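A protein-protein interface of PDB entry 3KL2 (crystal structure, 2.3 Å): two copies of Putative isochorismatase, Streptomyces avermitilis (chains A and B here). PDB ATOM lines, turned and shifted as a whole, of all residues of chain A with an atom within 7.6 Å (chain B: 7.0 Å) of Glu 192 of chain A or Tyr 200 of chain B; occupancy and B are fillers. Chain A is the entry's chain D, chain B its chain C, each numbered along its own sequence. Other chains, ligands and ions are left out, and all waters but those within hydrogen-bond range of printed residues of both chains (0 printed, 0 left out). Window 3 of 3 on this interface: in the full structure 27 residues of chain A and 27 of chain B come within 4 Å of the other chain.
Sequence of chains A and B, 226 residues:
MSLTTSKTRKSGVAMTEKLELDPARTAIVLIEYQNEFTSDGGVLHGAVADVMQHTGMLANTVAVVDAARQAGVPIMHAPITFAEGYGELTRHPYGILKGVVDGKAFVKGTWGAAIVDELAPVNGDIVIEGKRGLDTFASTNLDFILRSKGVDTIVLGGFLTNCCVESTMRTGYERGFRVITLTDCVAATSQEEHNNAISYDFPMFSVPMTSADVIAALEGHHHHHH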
ATOM      1  N   VAL A  51      24.380  -7.444   5.817  1.00  0.00           N
ATOM      2  CA  VAL A  51      24.233  -6.258   4.971  1.00  0.00           C
ATOM      3  C   VAL A  51      23.178  -5.249   5.515  1.00  0.00           C
ATOM      4  O   VAL A  51      23.389  -4.038   5.468  1.00  0.00           O
ATOM      5  CB  VAL A  51      23.928  -6.631   3.492  1.00  0.00           C
ATOM      6  CG1 VAL A  51      23.814  -5.362   2.631  1.00  0.00           C
ATOM      7  CG2 VAL A  51      25.033  -7.491   2.920  1.00  0.00           C
ATOM      8  N   ASN A 162      21.385  -6.858  -5.761  1.00  0.00           N
ATOM      9  CA  ASN A 162      21.785  -7.331  -7.079  1.00  0.00           C
ATOM     10  C   ASN A 162      20.756  -8.225  -7.829  1.00  0.00           C
ATOM     11  O   ASN A 162      21.045  -8.774  -8.887  1.00  0.00           O
ATOM     12  CB  ASN A 162      23.130  -8.067  -6.958  1.00  0.00           C
ATOM     13  CG  ASN A 162      23.033  -9.295  -6.141  1.00  0.00           C
ATOM     14  OD1 ASN A 162      22.346  -9.309  -5.125  1.00  0.00           O
ATOM     15  ND2 ASN A 162      23.675 -10.360  -6.593  1.00  0.00           N
ATOM     16  N   ALA A 188      21.468  -7.072   0.390  1.00  0.00           N
ATOM     17  CA  ALA A 188      21.663  -8.281  -0.389  1.00  0.00           C
ATOM     18  C   ALA A 188      22.199  -9.397   0.474  1.00  0.00           C
ATOM     19  O   ALA A 188      22.532  -9.171   1.615  1.00  0.00           O
ATOM     20  CB  ALA A 188      22.621  -8.013  -1.524  1.00  0.00           C
ATOM     21  N   THR A 189      22.303 -10.590  -0.095  1.00  0.00           N
ATOM     22  CA  THR A 189      22.826 -11.752   0.643  1.00  0.00           C
ATOM     23  C   THR A 189      24.333 -11.736   0.915  1.00  0.00           C
ATOM     24  O   THR A 189      24.839 -12.559   1.660  1.00  0.00           O
ATOM     25  CB  THR A 189      22.543 -13.055  -0.095  1.00  0.00           C
ATOM     26  OG1 THR A 189      23.361 -13.102  -1.271  1.00  0.00           O
ATOM     27  CG2 THR A 189      21.080 -13.126  -0.482  1.00  0.00           C
ATOM     28  N   SER A 190      25.067 -10.834   0.300  1.00  0.00           N
ATOM     29  CA  SER A 190      26.447 -10.658   0.677  1.00  0.00           C
ATOM     30  C   SER A 190      26.942  -9.259   0.332  1.00  0.00           C
ATOM     31  O   SER A 190      26.488  -8.642  -0.622  1.00  0.00           O
ATOM     32  CB  SER A 190      27.330 -11.747   0.059  1.00  0.00           C
ATOM     33  OG  SER A 190      27.611 -11.493  -1.293  1.00  0.00           O
ATOM     34  N   GLN A 191      27.876  -8.792   1.144  1.00  0.00           N
ATOM     35  CA  GLN A 191      28.412  -7.449   1.081  1.00  0.00           C
ATOM     36  C   GLN A 191      29.175  -7.223  -0.214  1.00  0.00           C
ATOM     37  O   GLN A 191      29.156  -6.139  -0.794  1.00  0.00           O
ATOM     38  CB  GLN A 191      29.377  -7.235   2.267  1.00  0.00           C
ATOM     39  CG  GLN A 191      29.732  -5.746   2.523  1.00  0.00           C
ATOM     40  CD  GLN A 191      28.537  -4.967   3.050  1.00  0.00           C
ATOM     41  OE1 GLN A 191      27.824  -5.449   3.938  1.00  0.00           O
ATOM     42  NE2 GLN A 191      28.307  -3.770   2.517  1.00  0.00           N
ATOM     43  N   GLU A 192      29.840  -8.272  -0.649  1.00  0.00           N
ATOM     44  CA  GLU A 192      30.527  -8.274  -1.907  1.00  0.00           C
ATOM     45  C   GLU A 192      29.533  -8.073  -3.066  1.00  0.00           C
ATOM     46  O   GLU A 192      29.706  -7.154  -3.857  1.00  0.00           O
ATOM     47  CB  GLU A 192      31.312  -9.586  -2.046  1.00  0.00           C
ATOM     48  CG  GLU A 192      32.502  -9.495  -2.918  1.00  0.00           C
ATOM     49  CD  GLU A 192      33.258 -10.815  -2.980  1.00  0.00           C
ATOM     50  OE1 GLU A 192      33.112 -11.634  -2.022  1.00  0.00           O
ATOM     51  OE2 GLU A 192      33.988 -11.028  -3.992  1.00  0.00           O
ATOM     52  N   GLU A 193      28.485  -8.904  -3.126  1.00  0.00           N
ATOM     53  CA  GLU A 193      27.491  -8.796  -4.181  1.00  0.00           C
ATOM     54  C   GLU A 193      26.911  -7.413  -4.087  1.00  0.00           C
ATOM     55  O   GLU A 193      26.615  -6.808  -5.109  1.00  0.00           O
ATOM     56  CB  GLU A 193      26.333  -9.789  -4.013  1.00  0.00           C
ATOM     57  CG  GLU A 193      26.652 -11.260  -4.270  1.00  0.00           C
ATOM     58  CD  GLU A 193      25.485 -12.191  -3.856  1.00  0.00           C
ATOM     59  OE1 GLU A 193      25.624 -12.902  -2.828  1.00  0.00           O
ATOM     60  OE2 GLU A 193      24.435 -12.216  -4.560  1.00  0.00           O
ATOM     61  N   HIS A 194      26.718  -6.923  -2.860  1.00  0.00           N
ATOM     62  CA  HIS A 194      25.997  -5.660  -2.644  1.00  0.00           C
ATOM     63  C   HIS A 194      26.791  -4.496  -3.189  1.00  0.00           C
ATOM     64  O   HIS A 194      26.253  -3.653  -3.940  1.00  0.00           O
ATOM     65  CB  HIS A 194      25.704  -5.490  -1.147  1.00  0.00           C
ATOM     66  CG  HIS A 194      25.242  -4.118  -0.749  1.00  0.00           C
ATOM     67  ND1 HIS A 194      23.916  -3.747  -0.762  1.00  0.00           N
ATOM     68  CD2 HIS A 194      25.919  -3.056  -0.258  1.00  0.00           C
ATOM     69  CE1 HIS A 194      23.803  -2.507  -0.331  1.00  0.00           C
ATOM     70  NE2 HIS A 194      25.002  -2.062  -0.018  1.00  0.00           N
ATOM     71  N   ASN A 195      28.080  -4.470  -2.814  1.00  0.00           N
ATOM     72  CA  ASN A 195      28.995  -3.387  -3.144  1.00  0.00           C
ATOM     73  C   ASN A 195      29.275  -3.269  -4.643  1.00  0.00           C
ATOM     74  O   ASN A 195      29.351  -2.176  -5.199  1.00  0.00           O
ATOM     75  CB  ASN A 195      30.330  -3.574  -2.390  1.00  0.00           C
ATOM     76  CG  ASN A 195      30.214  -3.279  -0.900  1.00  0.00           C
ATOM     77  OD1 ASN A 195      29.250  -2.678  -0.445  1.00  0.00           O
ATOM     78  ND2 ASN A 195      31.198  -3.701  -0.144  1.00  0.00           N
ATOM     79  N   ASN A 196      29.451  -4.412  -5.266  1.00  0.00           N
ATOM     80  CA  ASN A 196      29.719  -4.498  -6.675  1.00  0.00           C
ATOM     81  C   ASN A 196      28.508  -4.025  -7.457  1.00  0.00           C
ATOM     82  O   ASN A 196      28.665  -3.237  -8.379  1.00  0.00           O
ATOM     83  CB  ASN A 196      30.136  -5.930  -7.066  1.00  0.00           C
ATOM     84  CG  ASN A 196      31.496  -6.338  -6.467  1.00  0.00           C
ATOM     85  OD1 ASN A 196      32.253  -5.497  -5.918  1.00  0.00           O
ATOM     86  ND2 ASN A 196      31.829  -7.629  -6.599  1.00  0.00           N
ATOM     87  N   ALA A 197      27.298  -4.464  -7.085  1.00  0.00           N
ATOM     88  CA  ALA A 197      26.075  -3.991  -7.771  1.00  0.00           C
ATOM     89  C   ALA A 197      26.076  -2.472  -7.804  1.00  0.00           C
ATOM     90  O   ALA A 197      25.869  -1.849  -8.843  1.00  0.00           O
ATOM     91  CB  ALA A 197      24.803  -4.520  -7.066  1.00  0.00           C
ATOM     92  N   ILE A 198      26.359  -1.888  -6.646  1.00  0.00           N
ATOM     93  CA  ILE A 198      26.234  -0.458  -6.451  1.00  0.00           C
ATOM     94  C   ILE A 198      27.333   0.277  -7.212  1.00  0.00           C
ATOM     95  O   ILE A 198      27.081   1.322  -7.811  1.00  0.00           O
ATOM     96  CB  ILE A 198      26.251  -0.112  -4.929  1.00  0.00           C
ATOM     97  CG1 ILE A 198      24.883  -0.468  -4.300  1.00  0.00           C
ATOM     98  CG2 ILE A 198      26.673   1.357  -4.685  1.00  0.00           C
ATOM     99  CD1 ILE A 198      24.875  -0.510  -2.761  1.00  0.00           C
ATOM    100  N   TYR A 200      29.427  -0.911  -9.840  1.00  0.00           N
ATOM    101  CA  TYR A 200      29.467  -1.182 -11.287  1.00  0.00           C
ATOM    102  C   TYR A 200      28.165  -0.957 -12.046  1.00  0.00           C
ATOM    103  O   TYR A 200      28.198  -0.490 -13.169  1.00  0.00           O
ATOM    104  CB  TYR A 200      29.855  -2.645 -11.573  1.00  0.00           C
ATOM    105  CG  TYR A 200      31.139  -3.154 -10.899  1.00  0.00           C
ATOM    106  CD1 TYR A 200      32.256  -2.329 -10.729  1.00  0.00           C
ATOM    107  CD2 TYR A 200      31.244  -4.483 -10.490  1.00  0.00           C
ATOM    108  CE1 TYR A 200      33.421  -2.803 -10.149  1.00  0.00           C
ATOM    109  CE2 TYR A 200      32.411  -4.971  -9.897  1.00  0.00           C
ATOM    110  CZ  TYR A 200      33.499  -4.127  -9.717  1.00  0.00           C
ATOM    111  OH  TYR A 200      34.665  -4.622  -9.110  1.00  0.00           O
ATOM    112  N   ASN B 195      33.684 -10.737 -14.148  1.00  0.00           N
ATOM    113  CA  ASN B 195      33.774 -11.882 -13.241  1.00  0.00           C
ATOM    114  C   ASN B 195      32.637 -11.873 -12.185  1.00  0.00           C
ATOM    115  O   ASN B 195      32.088 -12.934 -11.853  1.00  0.00           O
ATOM    116  CB  ASN B 195      35.148 -11.955 -12.534  1.00  0.00           C
ATOM    117  CG  ASN B 195      36.283 -12.445 -13.441  1.00  0.00           C
ATOM    118  OD1 ASN B 195      36.081 -12.974 -14.517  1.00  0.00           O
ATOM    119  ND2 ASN B 195      37.489 -12.246 -12.986  1.00  0.00           N
ATOM    120  N   ASN B 196      32.308 -10.673 -11.702  1.00  0.00           N
ATOM    121  CA  ASN B 196      31.223 -10.455 -10.771  1.00  0.00           C
ATOM    122  C   ASN B 196      29.855 -10.948 -11.322  1.00  0.00           C
ATOM    123  O   ASN B 196      29.131 -11.693 -10.654  1.00  0.00           O
ATOM    124  CB  ASN B 196      31.147  -8.966 -10.398  1.00  0.00           C
ATOM    125  N   ALA B 197      29.545 -10.531 -12.539  1.00  0.00           N
ATOM    126  CA  ALA B 197      28.307 -10.868 -13.211  1.00  0.00           C
ATOM    127  C   ALA B 197      28.149 -12.381 -13.346  1.00  0.00           C
ATOM    128  O   ALA B 197      27.120 -12.951 -12.935  1.00  0.00           O
ATOM    129  CB  ALA B 197      28.250 -10.167 -14.598  1.00  0.00           C
ATOM    130  N   ILE B 198      29.190 -13.033 -13.859  1.00  0.00           N
ATOM    131  CA  ILE B 198      29.146 -14.457 -14.145  1.00  0.00           C
ATOM    132  C   ILE B 198      29.069 -15.285 -12.898  1.00  0.00           C
ATOM    133  O   ILE B 198      28.366 -16.294 -12.871  1.00  0.00           O
ATOM    134  CB  ILE B 198      30.386 -14.905 -14.955  1.00  0.00           C
ATOM    135  CG1 ILE B 198      30.223 -14.473 -16.426  1.00  0.00           C
ATOM    136  CG2 ILE B 198      30.638 -16.426 -14.812  1.00  0.00           C
ATOM    137  CD1 ILE B 198      31.548 -14.425 -17.207  1.00  0.00           C
ATOM    138  N   SER B 199      29.804 -14.868 -11.875  1.00  0.00           N
ATOM    139  CA  SER B 199      29.857 -15.615 -10.640  1.00  0.00           C
ATOM    140  C   SER B 199      28.587 -15.459  -9.787  1.00  0.00           C
ATOM    141  O   SER B 199      28.139 -16.443  -9.246  1.00  0.00           O
ATOM    142  CB  SER B 199      31.113 -15.235  -9.820  1.00  0.00           C
ATOM    143  OG  SER B 199      32.275 -15.673 -10.505  1.00  0.00           O
ATOM    144  N   TYR B 200      28.048 -14.244  -9.669  1.00  0.00           N
ATOM    145  CA  TYR B 200      26.930 -13.965  -8.787  1.00  0.00           C
ATOM    146  C   TYR B 200      25.569 -13.905  -9.474  1.00  0.00           C
ATOM    147  O   TYR B 200      24.599 -14.433  -8.944  1.00  0.00           O
ATOM    148  CB  TYR B 200      27.081 -12.612  -8.092  1.00  0.00           C
ATOM    149  CG  TYR B 200      28.400 -12.399  -7.394  1.00  0.00           C
ATOM    150  CD1 TYR B 200      29.064 -13.455  -6.765  1.00  0.00           C
ATOM    151  CD2 TYR B 200      28.989 -11.127  -7.369  1.00  0.00           C
ATOM    152  CE1 TYR B 200      30.309 -13.255  -6.145  1.00  0.00           C
ATOM    153  CE2 TYR B 200      30.215 -10.911  -6.744  1.00  0.00           C
ATOM    154  CZ  TYR B 200      30.869 -11.980  -6.131  1.00  0.00           C
ATOM    155  OH  TYR B 200      32.091 -11.766  -5.523  1.00  0.00           O
ATOM    156  N   ASP B 201      25.488 -13.225 -10.616  1.00  0.00           N
ATOM    157  CA  ASP B 201      24.190 -12.903 -11.233  1.00  0.00           C
ATOM    158  C   ASP B 201      23.768 -13.924 -12.269  1.00  0.00           C
ATOM    159  O   ASP B 201      22.578 -14.224 -12.377  1.00  0.00           O
ATOM    160  CB  ASP B 201      24.211 -11.505 -11.861  1.00  0.00           C
ATOM    161  CG  ASP B 201      24.477 -10.393 -10.846  1.00  0.00           C
ATOM    162  OD1 ASP B 201      24.299 -10.603  -9.626  1.00  0.00           O
ATOM    163  OD2 ASP B 201      24.858  -9.297 -11.281  1.00  0.00           O
ATOM    164  N   PHE B 202      24.710 -14.483 -13.027  1.00  0.00           N
ATOM    165  CA  PHE B 202      24.317 -15.417 -14.069  1.00  0.00           C
ATOM    166  C   PHE B 202      23.540 -16.624 -13.522  1.00  0.00           C
ATOM    167  O   PHE B 202      22.481 -16.974 -14.054  1.00  0.00           O
ATOM    168  CB  PHE B 202      25.504 -15.845 -14.930  1.00  0.00           C
ATOM    169  CG  PHE B 202      25.843 -14.886 -16.047  1.00  0.00           C
ATOM    170  CD1 PHE B 202      26.421 -15.349 -17.214  1.00  0.00           C
ATOM    171  CD2 PHE B 202      25.613 -13.529 -15.932  1.00  0.00           C
ATOM    172  CE1 PHE B 202      26.748 -14.475 -18.218  1.00  0.00           C
ATOM    173  CE2 PHE B 202      25.913 -12.657 -16.957  1.00  0.00           C
ATOM    174  CZ  PHE B 202      26.460 -13.122 -18.081  1.00  0.00           C
ATOM    175  N   PRO B 203      24.034 -17.245 -12.446  1.00  0.00           N
ATOM    176  CA  PRO B 203      23.337 -18.396 -11.830  1.00  0.00           C
ATOM    177  C   PRO B 203      21.921 -18.109 -11.333  1.00  0.00           C
ATOM    178  O   PRO B 203      21.125 -19.036 -11.243  1.00  0.00           O
ATOM    179  CB  PRO B 203      24.223 -18.735 -10.628  1.00  0.00           C
ATOM    180  CG  PRO B 203      25.607 -18.198 -11.027  1.00  0.00           C
ATOM    181  CD  PRO B 203      25.283 -16.918 -11.731  1.00  0.00           C
ATOM    182  N   MET B 204      21.624 -16.842 -11.025  1.00  0.00           N
ATOM    183  CA  MET B 204      20.272 -16.443 -10.606  1.00  0.00           C
ATOM    184  C   MET B 204      19.290 -16.565 -11.738  1.00  0.00           C
ATOM    185  O   MET B 204      18.164 -16.980 -11.511  1.00  0.00           O
ATOM    186  CB  MET B 204      20.229 -14.993 -10.072  1.00  0.00           C
ATOM    187  CG  MET B 204      20.832 -14.770  -8.638  1.00  0.00           C
ATOM    188  SD  MET B 204      20.969 -12.987  -8.217  1.00  0.00           S
ATOM    189  CE  MET B 204      20.530 -13.065  -6.519  1.00  0.00           C
ATOM    190  N   PHE B 205      19.685 -16.179 -12.953  1.00  0.00           N
ATOM    191  CA  PHE B 205      18.734 -16.049 -14.080  1.00  0.00           C
ATOM    192  C   PHE B 205      19.008 -16.921 -15.278  1.00  0.00           C
ATOM    193  O   PHE B 205      18.345 -16.760 -16.306  1.00  0.00           O
ATOM    194  CB  PHE B 205      18.660 -14.634 -14.586  1.00  0.00           C
ATOM    195  CG  PHE B 205      18.371 -13.588 -13.511  1.00  0.00           C
ATOM    196  CD1 PHE B 205      17.077 -13.185 -13.241  1.00  0.00           C
ATOM    197  CD2 PHE B 205      19.390 -13.019 -12.788  1.00  0.00           C
ATOM    198  CE1 PHE B 205      16.806 -12.209 -12.272  1.00  0.00           C
ATOM    199  CE2 PHE B 205      19.130 -12.056 -11.827  1.00  0.00           C
ATOM    200  CZ  PHE B 205      17.826 -11.638 -11.576  1.00  0.00           C
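Of chain B, only Tyr 200 (2.5 Å) comes within 4 Å of Glu 192 of chain A.
Tyr 200 of chain B touches three residues of chain A.
Printed residues of chain B within 4 Å of Glu 193 of chain A: Tyr 200 (3.8 Å).
Of the printed residues of chain B, Asn 162 of chain A touches Asp 201.
Of the printed residues of chain B, Asn 196 of chain A touches Tyr 200.
Printed residues of chain A within 4 Å of Asp 201 of chain B: Asn 162.
Phe 205 of chain B touches none of the printed residues of chain A.
Val 51 of chain A touches none of the printed residues of chain B.
The nearest residue of chain A that does not touch Tyr 200 of chain B is Asn 162 of chain A (4.3 Å).
The nearest printed residue of chain B that does not touch Glu 193 of chain A is Met 204 of chain B (4.5 Å).
Asn 196 of chain A touches Tyr 200 of chain B, but with the chains exchanged Tyr 200 of chain A does not touch Asn 196 of chain B (4.2 Å).
Of the 4 pairs that touch across the chains among the printed residues, none has its exchanged pair printed and touching as well.
The side-chain carboxylate of Glu 192 of chain A sits at hydrogen-bond distance from the side-chain hydroxyl of Tyr 200 of chain B.
ND2 of Asn 162 of chain A sits at hydrogen-bond distance from OD1 of Asp 201 of chain B (3.1 Å).
Printed residues of chain A that touch a printed residue of chain B: Asn 162, Glu 192, Glu 193 and Asn 196.
Among the printed residues, 4 pairs touch across the chains.
Among the printed residues, no Asp or Glu carboxylate lies within 4 Å of a Lys or Arg side-chain nitrogen of the other chain.
Glu 193 of chain A touches Tyr 200 of chain B (CG to CG, 3.8 Å).
ND2 of Asn 196 of chain A touches CE2 of Tyr 200 of chain B, at 3.7 Å.
ND2 of Asn 162 of chain A is in hydrogen-bond range of OE2 of Glu 193 of chain A (2.9 Å).
The side-chain hydroxyl (OG1) of Thr 189 of chain A lies within hydrogen-bond range of the side-chain carboxylate (OE1) of Glu 193 of chain A (2.8 Å).
OE1 of Glu 193 of chain A sits at hydrogen-bond distance from OG of Ser 190 of chain A (2.9 Å).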
